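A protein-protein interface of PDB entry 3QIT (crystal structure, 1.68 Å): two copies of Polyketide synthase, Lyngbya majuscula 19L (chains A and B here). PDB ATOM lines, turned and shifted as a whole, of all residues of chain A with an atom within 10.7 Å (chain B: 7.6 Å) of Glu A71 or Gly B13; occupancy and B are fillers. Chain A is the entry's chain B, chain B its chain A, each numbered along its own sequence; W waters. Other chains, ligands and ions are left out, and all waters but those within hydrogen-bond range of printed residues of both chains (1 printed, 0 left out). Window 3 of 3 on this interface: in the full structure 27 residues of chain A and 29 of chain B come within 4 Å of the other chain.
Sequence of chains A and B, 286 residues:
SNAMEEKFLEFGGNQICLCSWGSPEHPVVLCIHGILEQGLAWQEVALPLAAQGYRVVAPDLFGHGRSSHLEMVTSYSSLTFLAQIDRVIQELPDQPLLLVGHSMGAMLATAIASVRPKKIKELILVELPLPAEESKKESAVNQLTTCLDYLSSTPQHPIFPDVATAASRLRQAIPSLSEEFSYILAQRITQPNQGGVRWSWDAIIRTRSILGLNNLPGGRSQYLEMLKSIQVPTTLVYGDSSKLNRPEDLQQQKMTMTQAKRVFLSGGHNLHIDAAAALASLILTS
OE2 of Glu B10 lies within hydrogen-bond range of N of Gly B13 (3.0 Å).
The backbone carbonyl oxygen (O) of Gly B12 lies within hydrogen-bond range of the side-chain amide nitrogen (ND2) of Asn B14.
O of Gly A12 sits at hydrogen-bond distance from ND2 of Asn A14 (3.2 Å).
OH of Tyr A76 sits at hydrogen-bond distance from N of Leu A70, 2.9 Å away.
The side-chain hydroxyl of Ser A75 sits at hydrogen-bond distance from the backbone carbonyl oxygen of Met A72, at 3.0 Å.
The side-chain hydroxyl (OG1) of Thr A80 lies within hydrogen-bond range of the backbone carbonyl oxygen (O) of Ser A75.
Among the printed residues, merely in contact across the chains: Gly A12 with Glu B71, Gly A12 with Met B72, Gly A13 with Glu B71, Asn A14 with Met B72, Phe A62 with Met B72, Leu A70 with Met B72, Glu A71 with Gly B12, Glu A71 with Gly B13, Met A72 with Asn B14, Met A72 with Phe B62, Met A72 with Leu B70 and Thr A80 with Met B72.
Water W1 lies within hydrogen-bond range of the backbone carbonyl oxygen of Gly B13 (2.7 Å) and the side-chain carboxylate of Glu A71 (3.0 Å).
Gly A12 touches Glu B71, and with the chains exchanged Glu A71 touches Gly B12.
Gly A12 touches Met B72, and with the chains exchanged Met A72 touches Gly B12.
Phe A62 touches Met B72, and with the chains exchanged Met A72 touches Phe B62.
Leu A70 touches Met B72, and with the chains exchanged Met A72 touches Leu B70.
Positions printed for both chains: 11, 12, 13, 14, 15, 62, 68, 69, 70, 71 and 72.
Of the 13 pairs that touch across the chains among the printed residues, 12 have their exchanged pair printed and touching as well.
Of the 12 printed residues of chain B, 7 touch a printed residue of chain A.
Of the 25 printed residues of chain A, 8 touch a printed residue of chain B.
Of chain A, only Glu A71 comes within 4 Å of Gly B13.
Gly B12 touches just these residues of chain A: Glu A71 (3.3 Å) and Met A72 (3.5 Å).
Of chain A, only Met A72 (3.9 Å) comes within 4 Å of Asn B14.
Printed residues of chain A within 4 Å of Glu B71: Gly A12 and Gly A13.
Printed residues of chain B within 4 Å of Gly A12: Glu B71 (3.4 Å) and Met B72 (3.5 Å).
Of the printed residues of chain B, Gly A13 touches Glu B71 (3.99 Å).
Of the printed residues of chain A, Leu B70 touches Met A72 (3.8 Å).
Of the printed residues of chain A, Phe B62 touches Met A72.
Ser A153 touches none of the printed residues of chain B.
The backbone carbonyl oxygen of Gly B12 sits at hydrogen-bond distance from the backbone NH of Met A72, 3.5 Å away.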
ATOM      1  N   PHE A  11     -11.902 -30.421 -37.670  1.00  0.00           N
ATOM      2  CA  PHE A  11     -12.943 -30.597 -36.656  1.00  0.00           C
ATOM      3  C   PHE A  11     -12.850 -29.429 -35.709  1.00  0.00           C
ATOM      4  O   PHE A  11     -11.799 -29.196 -35.118  1.00  0.00           O
ATOM      5  CB  PHE A  11     -12.744 -31.913 -35.875  1.00  0.00           C
ATOM      6  CG  PHE A  11     -13.762 -32.123 -34.783  1.00  0.00           C
ATOM      7  CD1 PHE A  11     -15.112 -32.185 -35.095  1.00  0.00           C
ATOM      8  CD2 PHE A  11     -13.370 -32.262 -33.455  1.00  0.00           C
ATOM      9  CE1 PHE A  11     -16.083 -32.371 -34.088  1.00  0.00           C
ATOM     10  CE2 PHE A  11     -14.347 -32.461 -32.426  1.00  0.00           C
ATOM     11  CZ  PHE A  11     -15.683 -32.513 -32.757  1.00  0.00           C
ATOM     12  N   GLY A  12     -13.971 -28.722 -35.547  1.00  0.00           N
ATOM     13  CA  GLY A  12     -14.084 -27.646 -34.553  1.00  0.00           C
ATOM     14  C   GLY A  12     -13.081 -26.516 -34.750  1.00  0.00           C
ATOM     15  O   GLY A  12     -12.679 -25.871 -33.788  1.00  0.00           O
ATOM     16  N   GLY A  13     -12.648 -26.296 -35.990  1.00  0.00           N
ATOM     17  CA  GLY A  13     -11.667 -25.257 -36.268  1.00  0.00           C
ATOM     18  C   GLY A  13     -10.242 -25.719 -36.070  1.00  0.00           C
ATOM     19  O   GLY A  13      -9.315 -24.920 -36.122  1.00  0.00           O
ATOM     20  N   ASN A  14     -10.061 -27.022 -35.866  1.00  0.00           N
ATOM     21  CA  ASN A  14      -8.744 -27.573 -35.568  1.00  0.00           C
ATOM     22  C   ASN A  14      -8.457 -28.703 -36.543  1.00  0.00           C
ATOM     23  O   ASN A  14      -9.306 -29.038 -37.357  1.00  0.00           O
ATOM     24  CB  ASN A  14      -8.736 -28.106 -34.149  1.00  0.00           C
ATOM     25  CG  ASN A  14      -8.831 -27.006 -33.126  1.00  0.00           C
ATOM     26  OD1 ASN A  14      -7.885 -26.270 -32.936  1.00  0.00           O
ATOM     27  ND2 ASN A  14      -9.971 -26.906 -32.448  1.00  0.00           N
ATOM     28  N   GLN A  15      -7.259 -29.270 -36.470  1.00  0.00           N
ATOM     29  CA  GLN A  15      -6.900 -30.349 -37.415  1.00  0.00           C
ATOM     30  C   GLN A  15      -6.583 -31.603 -36.641  1.00  0.00           C
ATOM     31  O   GLN A  15      -5.783 -31.583 -35.697  1.00  0.00           O
ATOM     32  CB  GLN A  15      -5.693 -29.911 -38.243  1.00  0.00           C
ATOM     33  CG  GLN A  15      -5.988 -28.694 -39.133  1.00  0.00           C
ATOM     34  CD  GLN A  15      -6.885 -29.048 -40.300  1.00  0.00           C
ATOM     35  OE1 GLN A  15      -6.819 -30.155 -40.818  1.00  0.00           O
ATOM     36  NE2 GLN A  15      -7.739 -28.102 -40.719  1.00  0.00           N
ATOM     37  N   PHE A  62      -5.957 -34.277 -29.690  1.00  0.00           N
ATOM     38  CA  PHE A  62      -5.603 -32.843 -29.773  1.00  0.00           C
ATOM     39  C   PHE A  62      -4.495 -32.519 -28.782  1.00  0.00           C
ATOM     40  O   PHE A  62      -4.435 -33.095 -27.685  1.00  0.00           O
ATOM     41  CB  PHE A  62      -6.804 -31.930 -29.505  1.00  0.00           C
ATOM     42  CG  PHE A  62      -7.783 -31.836 -30.669  1.00  0.00           C
ATOM     43  CD1 PHE A  62      -7.347 -31.507 -31.953  1.00  0.00           C
ATOM     44  CD2 PHE A  62      -9.130 -32.049 -30.450  1.00  0.00           C
ATOM     45  CE1 PHE A  62      -8.292 -31.429 -33.043  1.00  0.00           C
ATOM     46  CE2 PHE A  62     -10.062 -31.958 -31.498  1.00  0.00           C
ATOM     47  CZ  PHE A  62      -9.638 -31.650 -32.795  1.00  0.00           C
ATOM     48  N   GLY A  63      -3.585 -31.645 -29.202  1.00  0.00           N
ATOM     49  CA  GLY A  63      -2.405 -31.313 -28.407  1.00  0.00           C
ATOM     50  C   GLY A  63      -1.264 -32.325 -28.438  1.00  0.00           C
ATOM     51  O   GLY A  63      -0.224 -32.087 -27.836  1.00  0.00           O
ATOM     52  N   SER A  67      -1.554 -33.397 -34.341  1.00  0.00           N
ATOM     53  CA  SER A  67      -2.850 -32.735 -34.272  1.00  0.00           C
ATOM     54  C   SER A  67      -2.709 -31.310 -33.705  1.00  0.00           C
ATOM     55  O   SER A  67      -1.731 -31.001 -33.010  1.00  0.00           O
ATOM     56  CB  SER A  67      -3.867 -33.516 -33.425  1.00  0.00           C
ATOM     57  OG  SER A  67      -4.334 -34.646 -34.135  1.00  0.00           O
ATOM     58  N   SER A  68      -3.679 -30.454 -34.025  1.00  0.00           N
ATOM     59  CA  SER A  68      -3.675 -29.063 -33.524  1.00  0.00           C
ATOM     60  C   SER A  68      -3.560 -28.969 -32.026  1.00  0.00           C
ATOM     61  O   SER A  68      -4.071 -29.819 -31.287  1.00  0.00           O
ATOM     62  CB  SER A  68      -4.985 -28.351 -33.901  1.00  0.00           C
ATOM     63  OG  SER A  68      -5.090 -28.284 -35.275  1.00  0.00           O
ATOM     64  N   HIS A  69      -2.920 -27.887 -31.579  1.00  0.00           N
ATOM     65  CA  HIS A  69      -3.024 -27.498 -30.165  1.00  0.00           C
ATOM     66  C   HIS A  69      -4.294 -26.670 -30.016  1.00  0.00           C
ATOM     67  O   HIS A  69      -4.643 -25.875 -30.921  1.00  0.00           O
ATOM     68  CB  HIS A  69      -1.820 -26.660 -29.746  1.00  0.00           C
ATOM     69  CG  HIS A  69      -0.518 -27.400 -29.798  1.00  0.00           C
ATOM     70  ND1 HIS A  69       0.652 -26.889 -29.276  1.00  0.00           N
ATOM     71  CD2 HIS A  69      -0.207 -28.616 -30.309  1.00  0.00           C
ATOM     72  CE1 HIS A  69       1.628 -27.760 -29.468  1.00  0.00           C
ATOM     73  NE2 HIS A  69       1.135 -28.810 -30.104  1.00  0.00           N
ATOM     74  N   LEU A  70      -4.958 -26.827 -28.869  1.00  0.00           N
ATOM     75  CA  LEU A  70      -6.172 -26.070 -28.595  1.00  0.00           C
ATOM     76  C   LEU A  70      -5.784 -24.740 -27.965  1.00  0.00           C
ATOM     77  O   LEU A  70      -5.203 -24.705 -26.873  1.00  0.00           O
ATOM     78  CB  LEU A  70      -7.147 -26.877 -27.721  1.00  0.00           C
ATOM     79  CG  LEU A  70      -7.456 -28.286 -28.292  1.00  0.00           C
ATOM     80  CD1 LEU A  70      -8.447 -29.037 -27.404  1.00  0.00           C
ATOM     81  CD2 LEU A  70      -8.019 -28.153 -29.723  1.00  0.00           C
ATOM     82  N   GLU A  71      -6.107 -23.645 -28.665  1.00  0.00           N
ATOM     83  CA  GLU A  71      -5.619 -22.317 -28.268  1.00  0.00           C
ATOM     84  C   GLU A  71      -6.234 -21.854 -26.970  1.00  0.00           C
ATOM     85  O   GLU A  71      -5.665 -21.032 -26.256  1.00  0.00           O
ATOM     86  CB  GLU A  71      -5.925 -21.265 -29.325  1.00  0.00           C
ATOM     87  CG  GLU A  71      -5.098 -21.349 -30.591  1.00  0.00           C
ATOM     88  CD  GLU A  71      -5.348 -20.136 -31.468  1.00  0.00           C
ATOM     89  OE1 GLU A  71      -6.197 -20.230 -32.368  1.00  0.00           O
ATOM     90  OE2 GLU A  71      -4.736 -19.079 -31.215  1.00  0.00           O
ATOM     91  N   MET A  72      -7.405 -22.371 -26.663  1.00  0.00           N
ATOM     92  CA  MET A  72      -7.954 -22.104 -25.333  1.00  0.00           C
ATOM     93  C   MET A  72      -7.807 -23.331 -24.446  1.00  0.00           C
ATOM     94  O   MET A  72      -8.429 -24.369 -24.699  1.00  0.00           O
ATOM     95  CB  MET A  72      -9.392 -21.678 -25.393  1.00  0.00           C
ATOM     96  CG  MET A  72      -9.817 -21.093 -24.020  1.00  0.00           C
ATOM     97  SD  MET A  72     -11.205 -20.080 -24.228  1.00  0.00           S
ATOM     98  CE  MET A  72     -12.320 -21.251 -24.988  1.00  0.00           C
ATOM     99  N   VAL A  73      -7.008 -23.179 -23.394  1.00  0.00           N
ATOM    100  CA  VAL A  73      -6.584 -24.309 -22.523  1.00  0.00           C
ATOM    101  C   VAL A  73      -7.742 -25.108 -21.928  1.00  0.00           C
ATOM    102  O   VAL A  73      -7.625 -26.320 -21.728  1.00  0.00           O
ATOM    103  CB  VAL A  73      -5.726 -23.793 -21.321  1.00  0.00           C
ATOM    104  CG1 VAL A  73      -5.293 -24.966 -20.431  1.00  0.00           C
ATOM    105  CG2 VAL A  73      -4.519 -23.041 -21.810  1.00  0.00           C
ATOM    106  N   THR A  74      -8.843 -24.421 -21.632  1.00  0.00           N
ATOM    107  CA  THR A  74     -10.025 -25.065 -21.051  1.00  0.00           C
ATOM    108  C   THR A  74     -10.716 -26.035 -22.007  1.00  0.00           C
ATOM    109  O   THR A  74     -11.603 -26.793 -21.609  1.00  0.00           O
ATOM    110  CB  THR A  74     -11.057 -24.043 -20.541  1.00  0.00           C
ATOM    111  OG1 THR A  74     -11.402 -23.131 -21.588  1.00  0.00           O
ATOM    112  CG2 THR A  74     -10.513 -23.292 -19.348  1.00  0.00           C
ATOM    113  N   SER A  75     -10.282 -26.012 -23.257  1.00  0.00           N
ATOM    114  CA  SER A  75     -10.793 -26.920 -24.297  1.00  0.00           C
ATOM    115  C   SER A  75     -10.289 -28.341 -24.096  1.00  0.00           C
ATOM    116  O   SER A  75     -10.899 -29.291 -24.605  1.00  0.00           O
ATOM    117  CB  SER A  75     -10.422 -26.410 -25.701  1.00  0.00           C
ATOM    118  OG  SER A  75     -11.028 -25.140 -25.956  1.00  0.00           O
ATOM    119  N   TYR A  76      -9.169 -28.499 -23.387  1.00  0.00           N
ATOM    120  CA  TYR A  76      -8.630 -29.838 -23.111  1.00  0.00           C
ATOM    121  C   TYR A  76      -9.441 -30.488 -21.998  1.00  0.00           C
ATOM    122  O   TYR A  76      -9.377 -30.079 -20.822  1.00  0.00           O
ATOM    123  CB  TYR A  76      -7.148 -29.767 -22.716  1.00  0.00           C
ATOM    124  CG  TYR A  76      -6.211 -29.438 -23.856  1.00  0.00           C
ATOM    125  CD1 TYR A  76      -5.997 -30.344 -24.892  1.00  0.00           C
ATOM    126  CD2 TYR A  76      -5.535 -28.220 -23.896  1.00  0.00           C
ATOM    127  CE1 TYR A  76      -5.127 -30.043 -25.936  1.00  0.00           C
ATOM    128  CE2 TYR A  76      -4.669 -27.894 -24.953  1.00  0.00           C
ATOM    129  CZ  TYR A  76      -4.483 -28.799 -25.965  1.00  0.00           C
ATOM    130  OH  TYR A  76      -3.592 -28.461 -26.961  1.00  0.00           O
ATOM    131  N   THR A  80     -13.966 -33.214 -24.829  1.00  0.00           N
ATOM    132  CA  THR A  80     -13.321 -32.837 -26.083  1.00  0.00           C
ATOM    133  C   THR A  80     -12.651 -34.023 -26.771  1.00  0.00           C
ATOM    134  O   THR A  80     -12.870 -34.250 -27.961  1.00  0.00           O
ATOM    135  CB  THR A  80     -12.299 -31.711 -25.868  1.00  0.00           C
ATOM    136  OG1 THR A  80     -13.001 -30.511 -25.510  1.00  0.00           O
ATOM    137  CG2 THR A  80     -11.462 -31.488 -27.133  1.00  0.00           C
ATOM    138  N   LEU A 151      -4.321 -23.048 -15.641  1.00  0.00           N
ATOM    139  CA  LEU A 151      -4.874 -22.643 -16.947  1.00  0.00           C
ATOM    140  C   LEU A 151      -4.274 -21.333 -17.474  1.00  0.00           C
ATOM    141  O   LEU A 151      -4.196 -21.123 -18.701  1.00  0.00           O
ATOM    142  CB  LEU A 151      -6.397 -22.491 -16.861  1.00  0.00           C
ATOM    143  CG  LEU A 151      -7.326 -23.678 -16.578  1.00  0.00           C
ATOM    144  CD1 LEU A 151      -8.702 -23.140 -16.249  1.00  0.00           C
ATOM    145  CD2 LEU A 151      -7.419 -24.644 -17.738  1.00  0.00           C
ATOM    146  N   SER A 152      -3.839 -20.460 -16.561  1.00  0.00           N
ATOM    147  CA  SER A 152      -3.312 -19.171 -16.982  1.00  0.00           C
ATOM    148  C   SER A 152      -1.798 -19.150 -16.923  1.00  0.00           C
ATOM    149  O   SER A 152      -1.172 -18.124 -17.206  1.00  0.00           O
ATOM    150  CB  SER A 152      -3.917 -18.024 -16.162  1.00  0.00           C
ATOM    151  OG  SER A 152      -3.695 -18.210 -14.788  1.00  0.00           O
ATOM    152  N   SER A 153      -1.205 -20.287 -16.569  1.00  0.00           N
ATOM    153  CA  SER A 153       0.239 -20.400 -16.600  1.00  0.00           C
ATOM    154  C   SER A 153       0.651 -20.686 -18.036  1.00  0.00           C
ATOM    155  O   SER A 153      -0.158 -21.073 -18.886  1.00  0.00           O
ATOM    156  CB  SER A 153       0.765 -21.457 -15.613  1.00  0.00           C
ATOM    157  OG  SER A 153       0.525 -22.781 -16.068  1.00  0.00           O
ATOM    158  N   THR A 154       1.907 -20.455 -18.331  1.00  0.00           N
ATOM    159  CA  THR A 154       2.353 -20.699 -19.691  1.00  0.00           C
ATOM    160  C   THR A 154       3.582 -21.583 -19.574  1.00  0.00           C
ATOM    161  O   THR A 154       4.709 -21.116 -19.789  1.00  0.00           O
ATOM    162  CB  THR A 154       2.656 -19.365 -20.407  1.00  0.00           C
ATOM    163  OG1 THR A 154       3.445 -18.545 -19.538  1.00  0.00           O
ATOM    164  CG2 THR A 154       1.371 -18.622 -20.752  1.00  0.00           C
ATOM    165  N   ASP A 202       1.575 -30.103 -26.860  1.00  0.00           N
ATOM    166  CA  ASP A 202       1.214 -28.887 -26.104  1.00  0.00           C
ATOM    167  C   ASP A 202       1.637 -29.012 -24.648  1.00  0.00           C
ATOM    168  O   ASP A 202       1.060 -29.807 -23.919  1.00  0.00           O
ATOM    169  CB  ASP A 202      -0.306 -28.667 -26.170  1.00  0.00           C
ATOM    170  CG  ASP A 202      -0.720 -27.274 -25.722  1.00  0.00           C
ATOM    171  OD1 ASP A 202       0.033 -26.637 -24.940  1.00  0.00           O
ATOM    172  OD2 ASP A 202      -1.807 -26.812 -26.150  1.00  0.00           O
ATOM    173  N   ILE A 204       0.912 -27.603 -22.009  1.00  0.00           N
ATOM    174  CA  ILE A 204      -0.128 -27.486 -20.969  1.00  0.00           C
ATOM    175  C   ILE A 204      -0.713 -28.848 -20.556  1.00  0.00           C
ATOM    176  O   ILE A 204      -1.225 -28.990 -19.443  1.00  0.00           O
ATOM    177  CB  ILE A 204      -1.241 -26.496 -21.399  1.00  0.00           C
ATOM    178  CG1 ILE A 204      -1.974 -25.935 -20.171  1.00  0.00           C
ATOM    179  CG2 ILE A 204      -2.200 -27.134 -22.397  1.00  0.00           C
ATOM    180  CD1 ILE A 204      -1.236 -24.779 -19.486  1.00  0.00           C
ATOM    181  N   ILE A 205      -0.595 -29.861 -21.421  1.00  0.00           N
ATOM    182  CA  ILE A 205      -1.232 -31.151 -21.209  1.00  0.00           C
ATOM    183  C   ILE A 205      -0.598 -31.941 -20.069  1.00  0.00           C
ATOM    184  O   ILE A 205      -1.253 -32.760 -19.429  1.00  0.00           O
ATOM    185  CB  ILE A 205      -1.222 -31.991 -22.507  1.00  0.00           C
ATOM    186  CG1 ILE A 205      -2.021 -31.275 -23.591  1.00  0.00           C
ATOM    187  CG2 ILE A 205      -1.824 -33.367 -22.265  1.00  0.00           C
ATOM    188  CD1 ILE A 205      -1.969 -31.939 -24.902  1.00  0.00           C
ATOM    189  N   GLU B  10      -8.080 -10.005 -26.244  1.00  0.00           N
ATOM    190  CA  GLU B  10      -7.766 -11.338 -26.769  1.00  0.00           C
ATOM    191  C   GLU B  10      -7.595 -12.307 -25.622  1.00  0.00           C
ATOM    192  O   GLU B  10      -7.022 -11.960 -24.594  1.00  0.00           O
ATOM    193  CB  GLU B  10      -6.460 -11.296 -27.588  1.00  0.00           C
ATOM    194  CG  GLU B  10      -6.123 -12.616 -28.349  1.00  0.00           C
ATOM    195  CD  GLU B  10      -5.394 -13.680 -27.505  1.00  0.00           C
ATOM    196  OE1 GLU B  10      -4.725 -13.306 -26.517  1.00  0.00           O
ATOM    197  OE2 GLU B  10      -5.464 -14.900 -27.839  1.00  0.00           O
ATOM    198  N   PHE B  11      -8.115 -13.520 -25.804  1.00  0.00           N
ATOM    199  CA  PHE B  11      -7.978 -14.589 -24.815  1.00  0.00           C
ATOM    200  C   PHE B  11      -8.192 -15.938 -25.461  1.00  0.00           C
ATOM    201  O   PHE B  11      -9.249 -16.190 -26.007  1.00  0.00           O
ATOM    202  CB  PHE B  11      -9.002 -14.417 -23.666  1.00  0.00           C
ATOM    203  CG  PHE B  11      -8.990 -15.542 -22.658  1.00  0.00           C
ATOM    204  CD1 PHE B  11      -7.842 -15.834 -21.937  1.00  0.00           C
ATOM    205  CD2 PHE B  11     -10.141 -16.308 -22.424  1.00  0.00           C
ATOM    206  CE1 PHE B  11      -7.828 -16.875 -21.012  1.00  0.00           C
ATOM    207  CE2 PHE B  11     -10.113 -17.372 -21.490  1.00  0.00           C
ATOM    208  CZ  PHE B  11      -8.969 -17.630 -20.789  1.00  0.00           C
ATOM    209  N   GLY B  12      -7.175 -16.801 -25.387  1.00  0.00           N
ATOM    210  CA  GLY B  12      -7.288 -18.188 -25.874  1.00  0.00           C
ATOM    211  C   GLY B  12      -7.600 -18.313 -27.366  1.00  0.00           C
ATOM    212  O   GLY B  12      -8.343 -19.222 -27.767  1.00  0.00           O
ATOM    213  N   GLY B  13      -7.072 -17.389 -28.175  1.00  0.00           N
ATOM    214  CA  GLY B  13      -7.339 -17.343 -29.615  1.00  0.00           C
ATOM    215  C   GLY B  13      -8.686 -16.744 -29.984  1.00  0.00           C
ATOM    216  O   GLY B  13      -9.059 -16.707 -31.155  1.00  0.00           O
ATOM    217  N   ASN B  14      -9.404 -16.262 -28.975  1.00  0.00           N
ATOM    218  CA  ASN B  14     -10.708 -15.679 -29.165  1.00  0.00           C
ATOM    219  C   ASN B  14     -10.695 -14.226 -28.705  1.00  0.00           C
ATOM    220  O   ASN B  14      -9.675 -13.737 -28.236  1.00  0.00           O
ATOM    221  CB  ASN B  14     -11.736 -16.461 -28.334  1.00  0.00           C
ATOM    222  CG  ASN B  14     -11.914 -17.875 -28.805  1.00  0.00           C
ATOM    223  OD1 ASN B  14     -12.321 -18.106 -29.922  1.00  0.00           O
ATOM    224  ND2 ASN B  14     -11.602 -18.844 -27.931  1.00  0.00           N
ATOM    225  N   GLN B  15     -11.833 -13.553 -28.845  1.00  0.00           N
ATOM    226  CA  GLN B  15     -11.983 -12.137 -28.457  1.00  0.00           C
ATOM    227  C   GLN B  15     -13.134 -11.968 -27.470  1.00  0.00           C
ATOM    228  O   GLN B  15     -14.265 -12.392 -27.722  1.00  0.00           O
ATOM    229  CB  GLN B  15     -12.249 -11.259 -29.703  1.00  0.00           C
ATOM    230  CG  GLN B  15     -11.092 -11.272 -30.738  1.00  0.00           C
ATOM    231  CD  GLN B  15      -9.858 -10.531 -30.262  1.00  0.00           C
ATOM    232  OE1 GLN B  15      -9.948  -9.464 -29.662  1.00  0.00           O
ATOM    233  NE2 GLN B  15      -8.697 -11.101 -30.516  1.00  0.00           N
ATOM    234  N   PHE B  62     -18.357 -15.737 -23.767  1.00  0.00           N
ATOM    235  CA  PHE B  62     -18.166 -16.342 -25.115  1.00  0.00           C
ATOM    236  C   PHE B  62     -19.483 -16.894 -25.646  1.00  0.00           C
ATOM    237  O   PHE B  62     -20.324 -17.410 -24.874  1.00  0.00           O
ATOM    238  CB  PHE B  62     -17.106 -17.433 -25.097  1.00  0.00           C
ATOM    239  CG  PHE B  62     -15.700 -16.905 -24.977  1.00  0.00           C
ATOM    240  CD1 PHE B  62     -15.209 -15.945 -25.866  1.00  0.00           C
ATOM    241  CD2 PHE B  62     -14.857 -17.417 -23.991  1.00  0.00           C
ATOM    242  CE1 PHE B  62     -13.883 -15.460 -25.734  1.00  0.00           C
ATOM    243  CE2 PHE B  62     -13.550 -16.957 -23.843  1.00  0.00           C
ATOM    244  CZ  PHE B  62     -13.046 -15.989 -24.733  1.00  0.00           C
ATOM    245  N   SER B  68     -16.455 -13.672 -29.285  1.00  0.00           N
ATOM    246  CA  SER B  68     -16.273 -14.810 -30.209  1.00  0.00           C
ATOM    247  C   SER B  68     -17.195 -15.965 -29.903  1.00  0.00           C
ATOM    248  O   SER B  68     -17.428 -16.297 -28.723  1.00  0.00           O
ATOM    249  CB  SER B  68     -14.858 -15.355 -30.098  1.00  0.00           C
ATOM    250  OG  SER B  68     -13.927 -14.385 -30.449  1.00  0.00           O
ATOM    251  N   HIS B  69     -17.651 -16.638 -30.962  1.00  0.00           N
ATOM    252  CA  HIS B  69     -18.236 -17.976 -30.781  1.00  0.00           C
ATOM    253  C   HIS B  69     -17.079 -18.961 -30.715  1.00  0.00           C
ATOM    254  O   HIS B  69     -16.048 -18.798 -31.395  1.00  0.00           O
ATOM    255  CB  HIS B  69     -19.163 -18.353 -31.924  1.00  0.00           C
ATOM    256  CG  HIS B  69     -20.324 -17.430 -32.091  1.00  0.00           C
ATOM    257  ND1 HIS B  69     -21.364 -17.705 -32.951  1.00  0.00           N
ATOM    258  CD2 HIS B  69     -20.644 -16.280 -31.454  1.00  0.00           C
ATOM    259  CE1 HIS B  69     -22.247 -16.727 -32.877  1.00  0.00           C
ATOM    260  NE2 HIS B  69     -21.825 -15.841 -31.995  1.00  0.00           N
ATOM    261  N   LEU B  70     -17.226 -19.985 -29.898  1.00  0.00           N
ATOM    262  CA  LEU B  70     -16.176 -21.007 -29.810  1.00  0.00           C
ATOM    263  C   LEU B  70     -16.383 -22.031 -30.926  1.00  0.00           C
ATOM    264  O   LEU B  70     -17.449 -22.626 -31.035  1.00  0.00           O
ATOM    265  CB  LEU B  70     -16.158 -21.655 -28.416  1.00  0.00           C
ATOM    266  CG  LEU B  70     -16.154 -20.639 -27.258  1.00  0.00           C
ATOM    267  CD1 LEU B  70     -16.244 -21.316 -25.907  1.00  0.00           C
ATOM    268  CD2 LEU B  70     -14.902 -19.767 -27.381  1.00  0.00           C
ATOM    269  N   GLU B  71     -15.368 -22.222 -31.764  1.00  0.00           N
ATOM    270  CA  GLU B  71     -15.522 -23.059 -32.959  1.00  0.00           C
ATOM    271  C   GLU B  71     -15.657 -24.542 -32.617  1.00  0.00           C
ATOM    272  O   GLU B  71     -16.223 -25.329 -33.393  1.00  0.00           O
ATOM    273  CB  GLU B  71     -14.347 -22.880 -33.936  1.00  0.00           C
ATOM    274  CG  GLU B  71     -14.110 -21.462 -34.414  1.00  0.00           C
ATOM    275  CD  GLU B  71     -13.010 -21.415 -35.475  1.00  0.00           C
ATOM    276  OE1 GLU B  71     -11.836 -21.183 -35.117  1.00  0.00           O
ATOM    277  OE2 GLU B  71     -13.320 -21.648 -36.657  1.00  0.00           O
ATOM    278  N   MET B  72     -15.133 -24.921 -31.464  1.00  0.00           N
ATOM    279  CA  MET B  72     -15.305 -26.300 -30.985  1.00  0.00           C
ATOM    280  C   MET B  72     -16.296 -26.314 -29.827  1.00  0.00           C
ATOM    281  O   MET B  72     -16.050 -25.703 -28.775  1.00  0.00           O
ATOM    282  CB  MET B  72     -13.988 -26.935 -30.593  1.00  0.00           C
ATOM    283  CG  MET B  72     -14.121 -28.458 -30.474  1.00  0.00           C
ATOM    284  SD  MET B  72     -12.513 -29.221 -30.443  1.00  0.00           S
ATOM    285  CE  MET B  72     -11.805 -28.433 -29.027  1.00  0.00           C
HETATM  286  O   HOH W   1      -7.489 -17.643 -33.085  1.00  0.00           O
